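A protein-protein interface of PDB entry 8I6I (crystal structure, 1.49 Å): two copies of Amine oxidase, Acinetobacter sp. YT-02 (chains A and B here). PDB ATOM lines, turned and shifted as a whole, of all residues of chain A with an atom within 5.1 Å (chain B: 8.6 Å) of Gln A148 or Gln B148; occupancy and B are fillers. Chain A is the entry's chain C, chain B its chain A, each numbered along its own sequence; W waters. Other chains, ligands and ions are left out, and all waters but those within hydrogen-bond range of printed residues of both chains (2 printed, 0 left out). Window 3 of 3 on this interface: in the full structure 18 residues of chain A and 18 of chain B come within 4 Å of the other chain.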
ATOM      1  N   GLY A 143      -4.153  13.585   2.701  1.00  0.00           N
ATOM      2  CA  GLY A 143      -4.998  13.168   3.829  1.00  0.00           C
ATOM      3  C   GLY A 143      -5.980  14.252   4.214  1.00  0.00           C
ATOM      4  O   GLY A 143      -6.750  14.041   5.144  1.00  0.00           O
ATOM      5  N   MET A 144      -6.004  15.373   3.491  1.00  0.00           N
ATOM      6  CA  MET A 144      -6.917  16.467   3.821  1.00  0.00           C
ATOM      7  C   MET A 144      -7.677  16.886   2.567  1.00  0.00           C
ATOM      8  O   MET A 144      -7.213  16.619   1.468  1.00  0.00           O
ATOM      9  CB  MET A 144      -6.181  17.669   4.417  1.00  0.00           C
ATOM     10  CG  MET A 144      -5.453  18.451   3.402  1.00  0.00           C
ATOM     11  SD  MET A 144      -4.411  19.761   4.181  1.00  0.00           S
ATOM     12  CE  MET A 144      -5.545  20.576   5.279  1.00  0.00           C
ATOM     13  N   THR A 145      -8.798  17.504   2.767  1.00  0.00           N
ATOM     14  CA  THR A 145      -9.675  18.030   1.691  1.00  0.00           C
ATOM     15  C   THR A 145      -9.285  19.457   1.322  1.00  0.00           C
ATOM     16  O   THR A 145      -8.638  20.142   2.083  1.00  0.00           O
ATOM     17  CB  THR A 145     -11.145  17.972   2.049  1.00  0.00           C
ATOM     18  OG1 THR A 145     -11.390  18.997   3.027  1.00  0.00           O
ATOM     19  CG2 THR A 145     -11.581  16.633   2.605  1.00  0.00           C
ATOM     20  N   VAL A 146      -9.693  19.885   0.150  1.00  0.00           N
ATOM     21  CA  VAL A 146      -9.490  21.310  -0.219  1.00  0.00           C
ATOM     22  C   VAL A 146     -10.190  22.169   0.794  1.00  0.00           C
ATOM     23  O   VAL A 146      -9.569  23.200   1.179  1.00  0.00           O
ATOM     24  CB  VAL A 146      -9.989  21.592  -1.638  1.00  0.00           C
ATOM     25  CG1 VAL A 146      -9.789  23.075  -1.938  1.00  0.00           C
ATOM     26  CG2 VAL A 146      -9.241  20.804  -2.665  1.00  0.00           C
ATOM     27  N   ALA A 147     -11.399  21.818   1.248  1.00  0.00           N
ATOM     28  CA  ALA A 147     -12.140  22.621   2.253  1.00  0.00           C
ATOM     29  C   ALA A 147     -11.267  22.819   3.492  1.00  0.00           C
ATOM     30  O   ALA A 147     -11.206  23.922   4.061  1.00  0.00           O
ATOM     31  CB  ALA A 147     -13.443  21.984   2.554  1.00  0.00           C
ATOM     32  N   GLN A 148     -10.615  21.769   3.959  1.00  0.00           N
ATOM     33  CA  GLN A 148      -9.749  21.828   5.160  1.00  0.00           C
ATOM     34  C   GLN A 148      -8.562  22.730   4.881  1.00  0.00           C
ATOM     35  O   GLN A 148      -8.150  23.514   5.788  1.00  0.00           O
ATOM     36  CB  GLN A 148      -9.353  20.409   5.573  1.00  0.00           C
ATOM     37  CG  GLN A 148     -10.544  19.669   6.165  1.00  0.00           C
ATOM     38  CD  GLN A 148     -10.304  18.196   6.385  1.00  0.00           C
ATOM     39  OE1 GLN A 148     -10.874  17.580   7.340  1.00  0.00           O
ATOM     40  NE2 GLN A 148      -9.424  17.641   5.625  1.00  0.00           N
ATOM     41  N   TRP A 149      -7.973  22.683   3.724  1.00  0.00           N
ATOM     42  CA  TRP A 149      -6.821  23.547   3.402  1.00  0.00           C
ATOM     43  C   TRP A 149      -7.318  24.981   3.363  1.00  0.00           C
ATOM     44  O   TRP A 149      -6.617  25.852   3.894  1.00  0.00           O
ATOM     45  CB  TRP A 149      -6.250  23.137   2.073  1.00  0.00           C
ATOM     46  CG  TRP A 149      -5.017  23.915   1.717  1.00  0.00           C
ATOM     47  CD1 TRP A 149      -3.737  23.583   1.965  1.00  0.00           C
ATOM     48  CD2 TRP A 149      -4.980  25.087   0.882  1.00  0.00           C
ATOM     49  NE1 TRP A 149      -2.873  24.514   1.411  1.00  0.00           N
ATOM     50  CE2 TRP A 149      -3.615  25.445   0.746  1.00  0.00           C
ATOM     51  CE3 TRP A 149      -5.949  25.889   0.280  1.00  0.00           C
ATOM     52  CZ2 TRP A 149      -3.217  26.551  -0.010  1.00  0.00           C
ATOM     53  CZ3 TRP A 149      -5.554  27.007  -0.413  1.00  0.00           C
ATOM     54  CH2 TRP A 149      -4.216  27.311  -0.568  1.00  0.00           C
ATOM     55  N   LEU A 150      -8.508  25.230   2.866  1.00  0.00           N
ATOM     56  CA  LEU A 150      -9.033  26.615   2.794  1.00  0.00           C
ATOM     57  C   LEU A 150      -9.263  27.108   4.230  1.00  0.00           C
ATOM     58  O   LEU A 150      -8.861  28.245   4.537  1.00  0.00           O
ATOM     59  CB  LEU A 150     -10.309  26.675   1.951  1.00  0.00           C
ATOM     60  CG  LEU A 150     -10.070  26.480   0.456  1.00  0.00           C
ATOM     61  CD1 LEU A 150     -11.388  26.295  -0.241  1.00  0.00           C
ATOM     62  CD2 LEU A 150      -9.284  27.650  -0.149  1.00  0.00           C
ATOM     63  N   ASP A 151      -9.767  26.272   5.119  1.00  0.00           N
ATOM     64  CA  ASP A 151     -10.010  26.677   6.527  1.00  0.00           C
ATOM     65  C   ASP A 151      -8.688  27.117   7.156  1.00  0.00           C
ATOM     66  O   ASP A 151      -8.702  28.047   7.985  1.00  0.00           O
ATOM     67  CB  ASP A 151     -10.496  25.488   7.343  1.00  0.00           C
ATOM     68  CG  ASP A 151     -11.907  25.023   7.106  1.00  0.00           C
ATOM     69  OD1 ASP A 151     -12.700  25.769   6.528  1.00  0.00           O
ATOM     70  OD2 ASP A 151     -12.185  23.857   7.477  1.00  0.00           O
ATOM     71  N   GLU A 152      -7.590  26.471   6.823  1.00  0.00           N
ATOM     72  CA  GLU A 152      -6.249  26.715   7.396  1.00  0.00           C
ATOM     73  C   GLU A 152      -5.586  27.933   6.731  1.00  0.00           C
ATOM     74  O   GLU A 152      -4.719  28.522   7.348  1.00  0.00           O
ATOM     75  CB  GLU A 152      -5.348  25.493   7.273  1.00  0.00           C
ATOM     76  CG  GLU A 152      -5.738  24.383   8.231  1.00  0.00           C
ATOM     77  CD  GLU A 152      -4.823  23.160   8.285  1.00  0.00           C
ATOM     78  OE1 GLU A 152      -3.856  23.070   7.509  1.00  0.00           O
ATOM     79  OE2 GLU A 152      -5.112  22.276   9.128  1.00  0.00           O
ATOM     80  N   ALA B 140     -20.420  17.990   9.433  1.00  0.00           N
ATOM     81  CA  ALA B 140     -19.075  18.134  10.046  1.00  0.00           C
ATOM     82  C   ALA B 140     -18.321  16.802  10.050  1.00  0.00           C
ATOM     83  O   ALA B 140     -17.154  16.819   9.627  1.00  0.00           O
ATOM     84  CB  ALA B 140     -19.166  18.687  11.443  1.00  0.00           C
ATOM     85  N   LEU B 141     -18.953  15.701  10.468  1.00  0.00           N
ATOM     86  CA  LEU B 141     -18.250  14.383  10.489  1.00  0.00           C
ATOM     87  C   LEU B 141     -17.965  13.921   9.050  1.00  0.00           C
ATOM     88  O   LEU B 141     -16.984  13.237   8.841  1.00  0.00           O
ATOM     89  CB  LEU B 141     -19.043  13.311  11.241  1.00  0.00           C
ATOM     90  CG  LEU B 141     -19.122  13.482  12.761  1.00  0.00           C
ATOM     91  CD1 LEU B 141     -20.199  12.566  13.351  1.00  0.00           C
ATOM     92  CD2 LEU B 141     -17.767  13.149  13.352  1.00  0.00           C
ATOM     93  N   ASP B 142     -18.821  14.288   8.115  1.00  0.00           N
ATOM     94  CA  ASP B 142     -18.677  13.821   6.717  1.00  0.00           C
ATOM     95  C   ASP B 142     -17.611  14.595   5.970  1.00  0.00           C
ATOM     96  O   ASP B 142     -17.256  14.194   4.856  1.00  0.00           O
ATOM     97  CB  ASP B 142     -19.983  13.895   5.956  1.00  0.00           C
ATOM     98  CG  ASP B 142     -20.039  12.929   4.795  1.00  0.00           C
ATOM     99  OD1 ASP B 142     -19.466  11.823   4.930  1.00  0.00           O
ATOM    100  OD2 ASP B 142     -20.725  13.245   3.811  1.00  0.00           O
ATOM    101  N   GLY B 143     -17.094  15.669   6.535  1.00  0.00           N
ATOM    102  CA  GLY B 143     -16.039  16.459   5.914  1.00  0.00           C
ATOM    103  C   GLY B 143     -14.667  16.085   6.430  1.00  0.00           C
ATOM    104  O   GLY B 143     -13.704  16.699   6.046  1.00  0.00           O
ATOM    105  N   MET B 144     -14.567  15.091   7.301  1.00  0.00           N
ATOM    106  CA  MET B 144     -13.265  14.679   7.845  1.00  0.00           C
ATOM    107  C   MET B 144     -13.129  13.172   7.731  1.00  0.00           C
ATOM    108  O   MET B 144     -14.151  12.472   7.526  1.00  0.00           O
ATOM    109  CB  MET B 144     -13.123  15.152   9.293  1.00  0.00           C
ATOM    110  CG  MET B 144     -13.974  14.367  10.170  1.00  0.00           C
ATOM    111  SD  MET B 144     -13.992  14.992  11.921  1.00  0.00           S
ATOM    112  CE  MET B 144     -12.311  14.822  12.433  1.00  0.00           C
ATOM    113  N   THR B 145     -11.897  12.714   7.763  1.00  0.00           N
ATOM    114  CA  THR B 145     -11.539  11.297   7.646  1.00  0.00           C
ATOM    115  C   THR B 145     -11.525  10.659   9.034  1.00  0.00           C
ATOM    116  O   THR B 145     -11.362  11.353  10.076  1.00  0.00           O
ATOM    117  CB  THR B 145     -10.220  11.087   6.942  1.00  0.00           C
ATOM    118  OG1 THR B 145      -9.179  11.502   7.846  1.00  0.00           O
ATOM    119  CG2 THR B 145     -10.141  11.776   5.612  1.00  0.00           C
ATOM    120  N   VAL B 146     -11.559   9.320   9.064  1.00  0.00           N
ATOM    121  CA  VAL B 146     -11.366   8.611  10.341  1.00  0.00           C
ATOM    122  C   VAL B 146      -9.980   8.931  10.908  1.00  0.00           C
ATOM    123  O   VAL B 146      -9.866   9.082  12.141  1.00  0.00           O
ATOM    124  CB  VAL B 146     -11.572   7.098  10.166  1.00  0.00           C
ATOM    125  CG1 VAL B 146     -11.318   6.438  11.510  1.00  0.00           C
ATOM    126  CG2 VAL B 146     -12.953   6.811   9.605  1.00  0.00           C
ATOM    127  N   ALA B 147      -8.971   9.045  10.054  1.00  0.00           N
ATOM    128  CA  ALA B 147      -7.604   9.333  10.521  1.00  0.00           C
ATOM    129  C   ALA B 147      -7.606  10.666  11.268  1.00  0.00           C
ATOM    130  O   ALA B 147      -6.939  10.761  12.292  1.00  0.00           O
ATOM    131  CB  ALA B 147      -6.669   9.319   9.372  1.00  0.00           C
ATOM    132  N   GLN B 148      -8.341  11.669  10.772  1.00  0.00           N
ATOM    133  CA  GLN B 148      -8.363  13.005  11.412  1.00  0.00           C
ATOM    134  C   GLN B 148      -9.139  12.888  12.715  1.00  0.00           C
ATOM    135  O   GLN B 148      -8.748  13.542  13.694  1.00  0.00           O
ATOM    136  CB  GLN B 148      -8.997  13.997  10.430  1.00  0.00           C
ATOM    137  CG  GLN B 148      -8.110  14.268   9.247  1.00  0.00           C
ATOM    138  CD  GLN B 148      -8.756  15.091   8.153  1.00  0.00           C
ATOM    139  OE1 GLN B 148      -8.043  15.809   7.414  1.00  0.00           O
ATOM    140  NE2 GLN B 148     -10.048  14.979   8.018  1.00  0.00           N
ATOM    141  N   TRP B 149     -10.188  12.107  12.754  1.00  0.00           N
ATOM    142  CA  TRP B 149     -10.946  11.897  14.019  1.00  0.00           C
ATOM    143  C   TRP B 149      -9.996  11.241  15.032  1.00  0.00           C
ATOM    144  O   TRP B 149      -9.973  11.632  16.231  1.00  0.00           O
ATOM    145  CB  TRP B 149     -12.188  11.060  13.759  1.00  0.00           C
ATOM    146  CG  TRP B 149     -13.059  10.908  14.967  1.00  0.00           C
ATOM    147  CD1 TRP B 149     -14.102  11.716  15.335  1.00  0.00           C
ATOM    148  CD2 TRP B 149     -13.013   9.864  15.951  1.00  0.00           C
ATOM    149  NE1 TRP B 149     -14.668  11.264  16.508  1.00  0.00           N
ATOM    150  CE2 TRP B 149     -14.057  10.116  16.876  1.00  0.00           C
ATOM    151  CE3 TRP B 149     -12.219   8.728  16.115  1.00  0.00           C
ATOM    152  CZ2 TRP B 149     -14.309   9.262  17.960  1.00  0.00           C
ATOM    153  CZ3 TRP B 149     -12.471   7.889  17.185  1.00  0.00           C
ATOM    154  CH2 TRP B 149     -13.470   8.180  18.111  1.00  0.00           C
ATOM    155  N   LEU B 150      -9.264  10.227  14.627  1.00  0.00           N
ATOM    156  CA  LEU B 150      -8.312   9.586  15.546  1.00  0.00           C
ATOM    157  C   LEU B 150      -7.300  10.623  16.056  1.00  0.00           C
ATOM    158  O   LEU B 150      -6.980  10.567  17.268  1.00  0.00           O
ATOM    159  CB  LEU B 150      -7.684   8.378  14.862  1.00  0.00           C
ATOM    160  CG  LEU B 150      -8.622   7.215  14.631  1.00  0.00           C
ATOM    161  CD1 LEU B 150      -7.955   6.189  13.716  1.00  0.00           C
ATOM    162  CD2 LEU B 150      -9.070   6.564  15.939  1.00  0.00           C
ATOM    163  N   ASP B 151      -6.754  11.465  15.203  1.00  0.00           N
ATOM    164  CA  ASP B 151      -5.776  12.501  15.636  1.00  0.00           C
ATOM    165  C   ASP B 151      -6.388  13.364  16.749  1.00  0.00           C
ATOM    166  O   ASP B 151      -5.645  13.795  17.691  1.00  0.00           O
ATOM    167  CB  ASP B 151      -5.465  13.439  14.472  1.00  0.00           C
ATOM    168  CG  ASP B 151      -4.535  12.896  13.435  1.00  0.00           C
ATOM    169  OD1 ASP B 151      -3.938  11.832  13.686  1.00  0.00           O
ATOM    170  OD2 ASP B 151      -4.413  13.565  12.372  1.00  0.00           O
ATOM    171  N   GLU B 152      -7.673  13.657  16.670  1.00  0.00           N
ATOM    172  CA  GLU B 152      -8.373  14.516  17.666  1.00  0.00           C
ATOM    173  C   GLU B 152      -8.802  13.762  18.930  1.00  0.00           C
ATOM    174  O   GLU B 152      -9.060  14.432  19.974  1.00  0.00           O
ATOM    175  CB  GLU B 152      -9.591  15.171  17.011  1.00  0.00           C
ATOM    176  CG  GLU B 152      -9.181  16.150  15.931  1.00  0.00           C
ATOM    177  CD  GLU B 152     -10.277  16.890  15.168  1.00  0.00           C
ATOM    178  OE1 GLU B 152     -11.477  16.734  15.460  1.00  0.00           O
ATOM    179  OE2 GLU B 152      -9.902  17.627  14.224  1.00  0.00           O
ATOM    180  N   ASN B 153      -9.045  12.458  18.850  1.00  0.00           N
ATOM    181  CA  ASN B 153      -9.780  11.727  19.916  1.00  0.00           C
ATOM    182  C   ASN B 153      -8.893  10.700  20.622  1.00  0.00           C
ATOM    183  O   ASN B 153      -9.282  10.255  21.738  1.00  0.00           O
ATOM    184  CB  ASN B 153     -11.044  11.069  19.377  1.00  0.00           C
ATOM    185  CG  ASN B 153     -12.146  12.058  19.101  1.00  0.00           C
ATOM    186  OD1 ASN B 153     -12.971  12.310  19.987  1.00  0.00           O
ATOM    187  ND2 ASN B 153     -12.118  12.713  17.942  1.00  0.00           N
ATOM    188  N   VAL B 154      -7.807  10.261  19.999  1.00  0.00           N
ATOM    189  CA  VAL B 154      -6.987   9.142  20.524  1.00  0.00           C
ATOM    190  C   VAL B 154      -5.562   9.613  20.676  1.00  0.00           C
ATOM    191  O   VAL B 154      -4.990  10.199  19.735  1.00  0.00           O
ATOM    192  CB  VAL B 154      -7.084   7.916  19.598  1.00  0.00           C
ATOM    193  CG1 VAL B 154      -6.021   6.868  19.941  1.00  0.00           C
ATOM    194  CG2 VAL B 154      -8.488   7.343  19.587  1.00  0.00           C
ATOM    195  N   THR B 175      -7.827   4.553   7.055  1.00  0.00           N
ATOM    196  CA  THR B 175      -8.485   5.608   7.878  1.00  0.00           C
ATOM    197  C   THR B 175      -8.389   6.965   7.178  1.00  0.00           C
ATOM    198  O   THR B 175      -9.229   7.798   7.439  1.00  0.00           O
ATOM    199  CB  THR B 175      -7.813   5.672   9.267  1.00  0.00           C
ATOM    200  OG1 THR B 175      -6.413   5.850   9.072  1.00  0.00           O
ATOM    201  CG2 THR B 175      -8.082   4.428  10.086  1.00  0.00           C
ATOM    202  N   THR B 176      -7.410   7.172   6.278  1.00  0.00           N
ATOM    203  CA  THR B 176      -7.299   8.466   5.541  1.00  0.00           C
ATOM    204  C   THR B 176      -8.255   8.489   4.360  1.00  0.00           C
ATOM    205  O   THR B 176      -8.372   9.542   3.736  1.00  0.00           O
ATOM    206  CB  THR B 176      -5.895   8.633   5.014  1.00  0.00           C
ATOM    207  OG1 THR B 176      -5.674   7.536   4.122  1.00  0.00           O
ATOM    208  CG2 THR B 176      -4.853   8.713   6.091  1.00  0.00           C
ATOM    209  N   GLU B 177      -8.918   7.373   4.058  1.00  0.00           N
ATOM    210  CA  GLU B 177      -9.802   7.241   2.866  1.00  0.00           C
ATOM    211  C   GLU B 177     -11.280   7.313   3.218  1.00  0.00           C
ATOM    212  O   GLU B 177     -12.107   7.663   2.344  1.00  0.00           O
ATOM    213  CB  GLU B 177      -9.509   5.924   2.153  1.00  0.00           C
ATOM    214  CG  GLU B 177      -8.115   5.844   1.581  1.00  0.00           C
ATOM    215  CD  GLU B 177      -7.640   4.440   1.208  1.00  0.00           C
ATOM    216  OE1 GLU B 177      -6.554   4.404   0.574  1.00  0.00           O
ATOM    217  OE2 GLU B 177      -8.373   3.450   1.432  1.00  0.00           O
ATOM    218  N   VAL B 178     -11.664   6.958   4.432  1.00  0.00           N
ATOM    219  CA  VAL B 178     -13.066   6.754   4.800  1.00  0.00           C
ATOM    220  C   VAL B 178     -13.557   7.992   5.548  1.00  0.00           C
ATOM    221  O   VAL B 178     -12.898   8.465   6.479  1.00  0.00           O
ATOM    222  CB  VAL B 178     -13.243   5.505   5.681  1.00  0.00           C
ATOM    223  CG1 VAL B 178     -14.719   5.355   6.071  1.00  0.00           C
ATOM    224  CG2 VAL B 178     -12.692   4.231   5.025  1.00  0.00           C
ATOM    225  N   SER B 179     -14.713   8.507   5.178  1.00  0.00           N
ATOM    226  CA  SER B 179     -15.389   9.580   5.913  1.00  0.00           C
ATOM    227  C   SER B 179     -15.632   9.140   7.363  1.00  0.00           C
ATOM    228  O   SER B 179     -16.143   8.024   7.602  1.00  0.00           O
ATOM    229  CB  SER B 179     -16.686   9.852   5.271  1.00  0.00           C
ATOM    230  OG  SER B 179     -17.605  10.486   6.131  1.00  0.00           O
ATOM    231  N   MET B 180     -15.355  10.026   8.307  1.00  0.00           N
ATOM    232  CA  MET B 180     -15.693   9.692   9.692  1.00  0.00           C
ATOM    233  C   MET B 180     -17.197   9.556   9.856  1.00  0.00           C
ATOM    234  O   MET B 180     -17.637   8.676  10.653  1.00  0.00           O
ATOM    235  CB  MET B 180     -15.156  10.747  10.660  1.00  0.00           C
ATOM    236  CG  MET B 180     -15.415  10.409  12.094  1.00  0.00           C
ATOM    237  SD  MET B 180     -14.611   8.857  12.618  1.00  0.00           S
ATOM    238  CE  MET B 180     -15.514   8.451  14.106  1.00  0.00           C
ATOM    239  N   THR B 398     -15.176  11.286   1.953  1.00  0.00           N
ATOM    240  CA  THR B 398     -15.763  12.534   2.475  1.00  0.00           C
ATOM    241  C   THR B 398     -16.810  13.103   1.518  1.00  0.00           C
ATOM    242  O   THR B 398     -16.664  13.085   0.272  1.00  0.00           O
ATOM    243  CB  THR B 398     -14.680  13.558   2.809  1.00  0.00           C
ATOM    244  OG1 THR B 398     -13.901  13.896   1.659  1.00  0.00           O
ATOM    245  CG2 THR B 398     -13.804  13.171   3.970  1.00  0.00           C
HETATM  246  O   HOH W   1      -6.776  11.846   6.708  1.00  0.00           O
HETATM  247  O   HOH W   2     -13.748  18.838   4.296  1.00  0.00           O
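O of Gly B143 sits close to OE1 of Gln A148 (3.2 Å).
OE1 of Gln B148 sits close to O of Gly A143, 3.2 Å away.
The side-chain amide nitrogen (NE2) of Gln B148 is in hydrogen-bond range of the side-chain amide oxygen (OE1) of Gln A148, at 2.8 Å.
The backbone carbonyl oxygen (O) of Met B144 sits at hydrogen-bond distance from the backbone NH (N) of Met B180 (2.8 Å).
The side-chain amide nitrogen (NE2) of Gln B148 sits close to the backbone NH (N) of Thr B145 (2.9 Å).
The side-chain hydroxyl (OG1) of Thr A145 sits close to the backbone NH (N) of Ala A147.
NE2 of Gln A148 sits close to N of Thr A145, at 2.9 Å.
Among the printed residues, merely in contact across the chains: Thr A145 with Thr B398, Gln A148 with Met B144 and Met A144 with Gln B148.
Gln A148 touches three residues of chain B.
Of chain B, only Thr B398 (3.7 Å) comes within 4 Å of Thr A145.
Ala A147 touches none of the printed residues of chain B.
Printed residues of chain B within 4 Å of Gly A143: Gln B148.
Printed residues of chain A within 4 Å of Thr B398: Thr A145 (3.7 Å).
Printed residues of chain A within 4 Å of Gly B143: Gln A148 (3.2 Å).
Of the printed residues of chain B, Met A144 touches Gln B148 (3.8 Å).
Of the printed residues of chain A, Met B144 touches Gln A148.
Trp B149 touches none of the printed residues of chain A.
Ala B147 touches none of the printed residues of chain A.
The nearest residue of chain B that does not touch Gln A148 is Thr B145 (5.0 Å).
The nearest residue of chain A that does not touch Gln B148 is Thr A145 (5.0 Å).
The nearest printed residue of chain B that does not touch Gly A143 is Thr B145 (4.1 Å).
Hydrophobic or aromatic side chains of chain A within 4 Å of the printed part of chain B: Met A144.
Among the printed residues, 6 pairs touch across the chains.
Among the printed residues, no Asp or Glu carboxylate lies within 4 Å of a Lys or Arg side-chain nitrogen of the other chain.
Gly A143 touches Gln B148, and with the chains exchanged Gln A148 touches Gly B143.
Met A144 touches Gln B148, and with the chains exchanged Gln A148 touches Met B144.
Gln B148 touches its own counterpart, Gln A148.
Of the 6 pairs that touch across the chains among the printed residues, 5 have their exchanged pair printed and touching as well.
Water W1 bridges OG1 of Thr B145 (2.7 Å) and O of Gly A143 (2.7 Å).
Water W2 bridges OG1 of Thr A145 (2.7 Å) and O of Gly B143 (2.8 Å).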
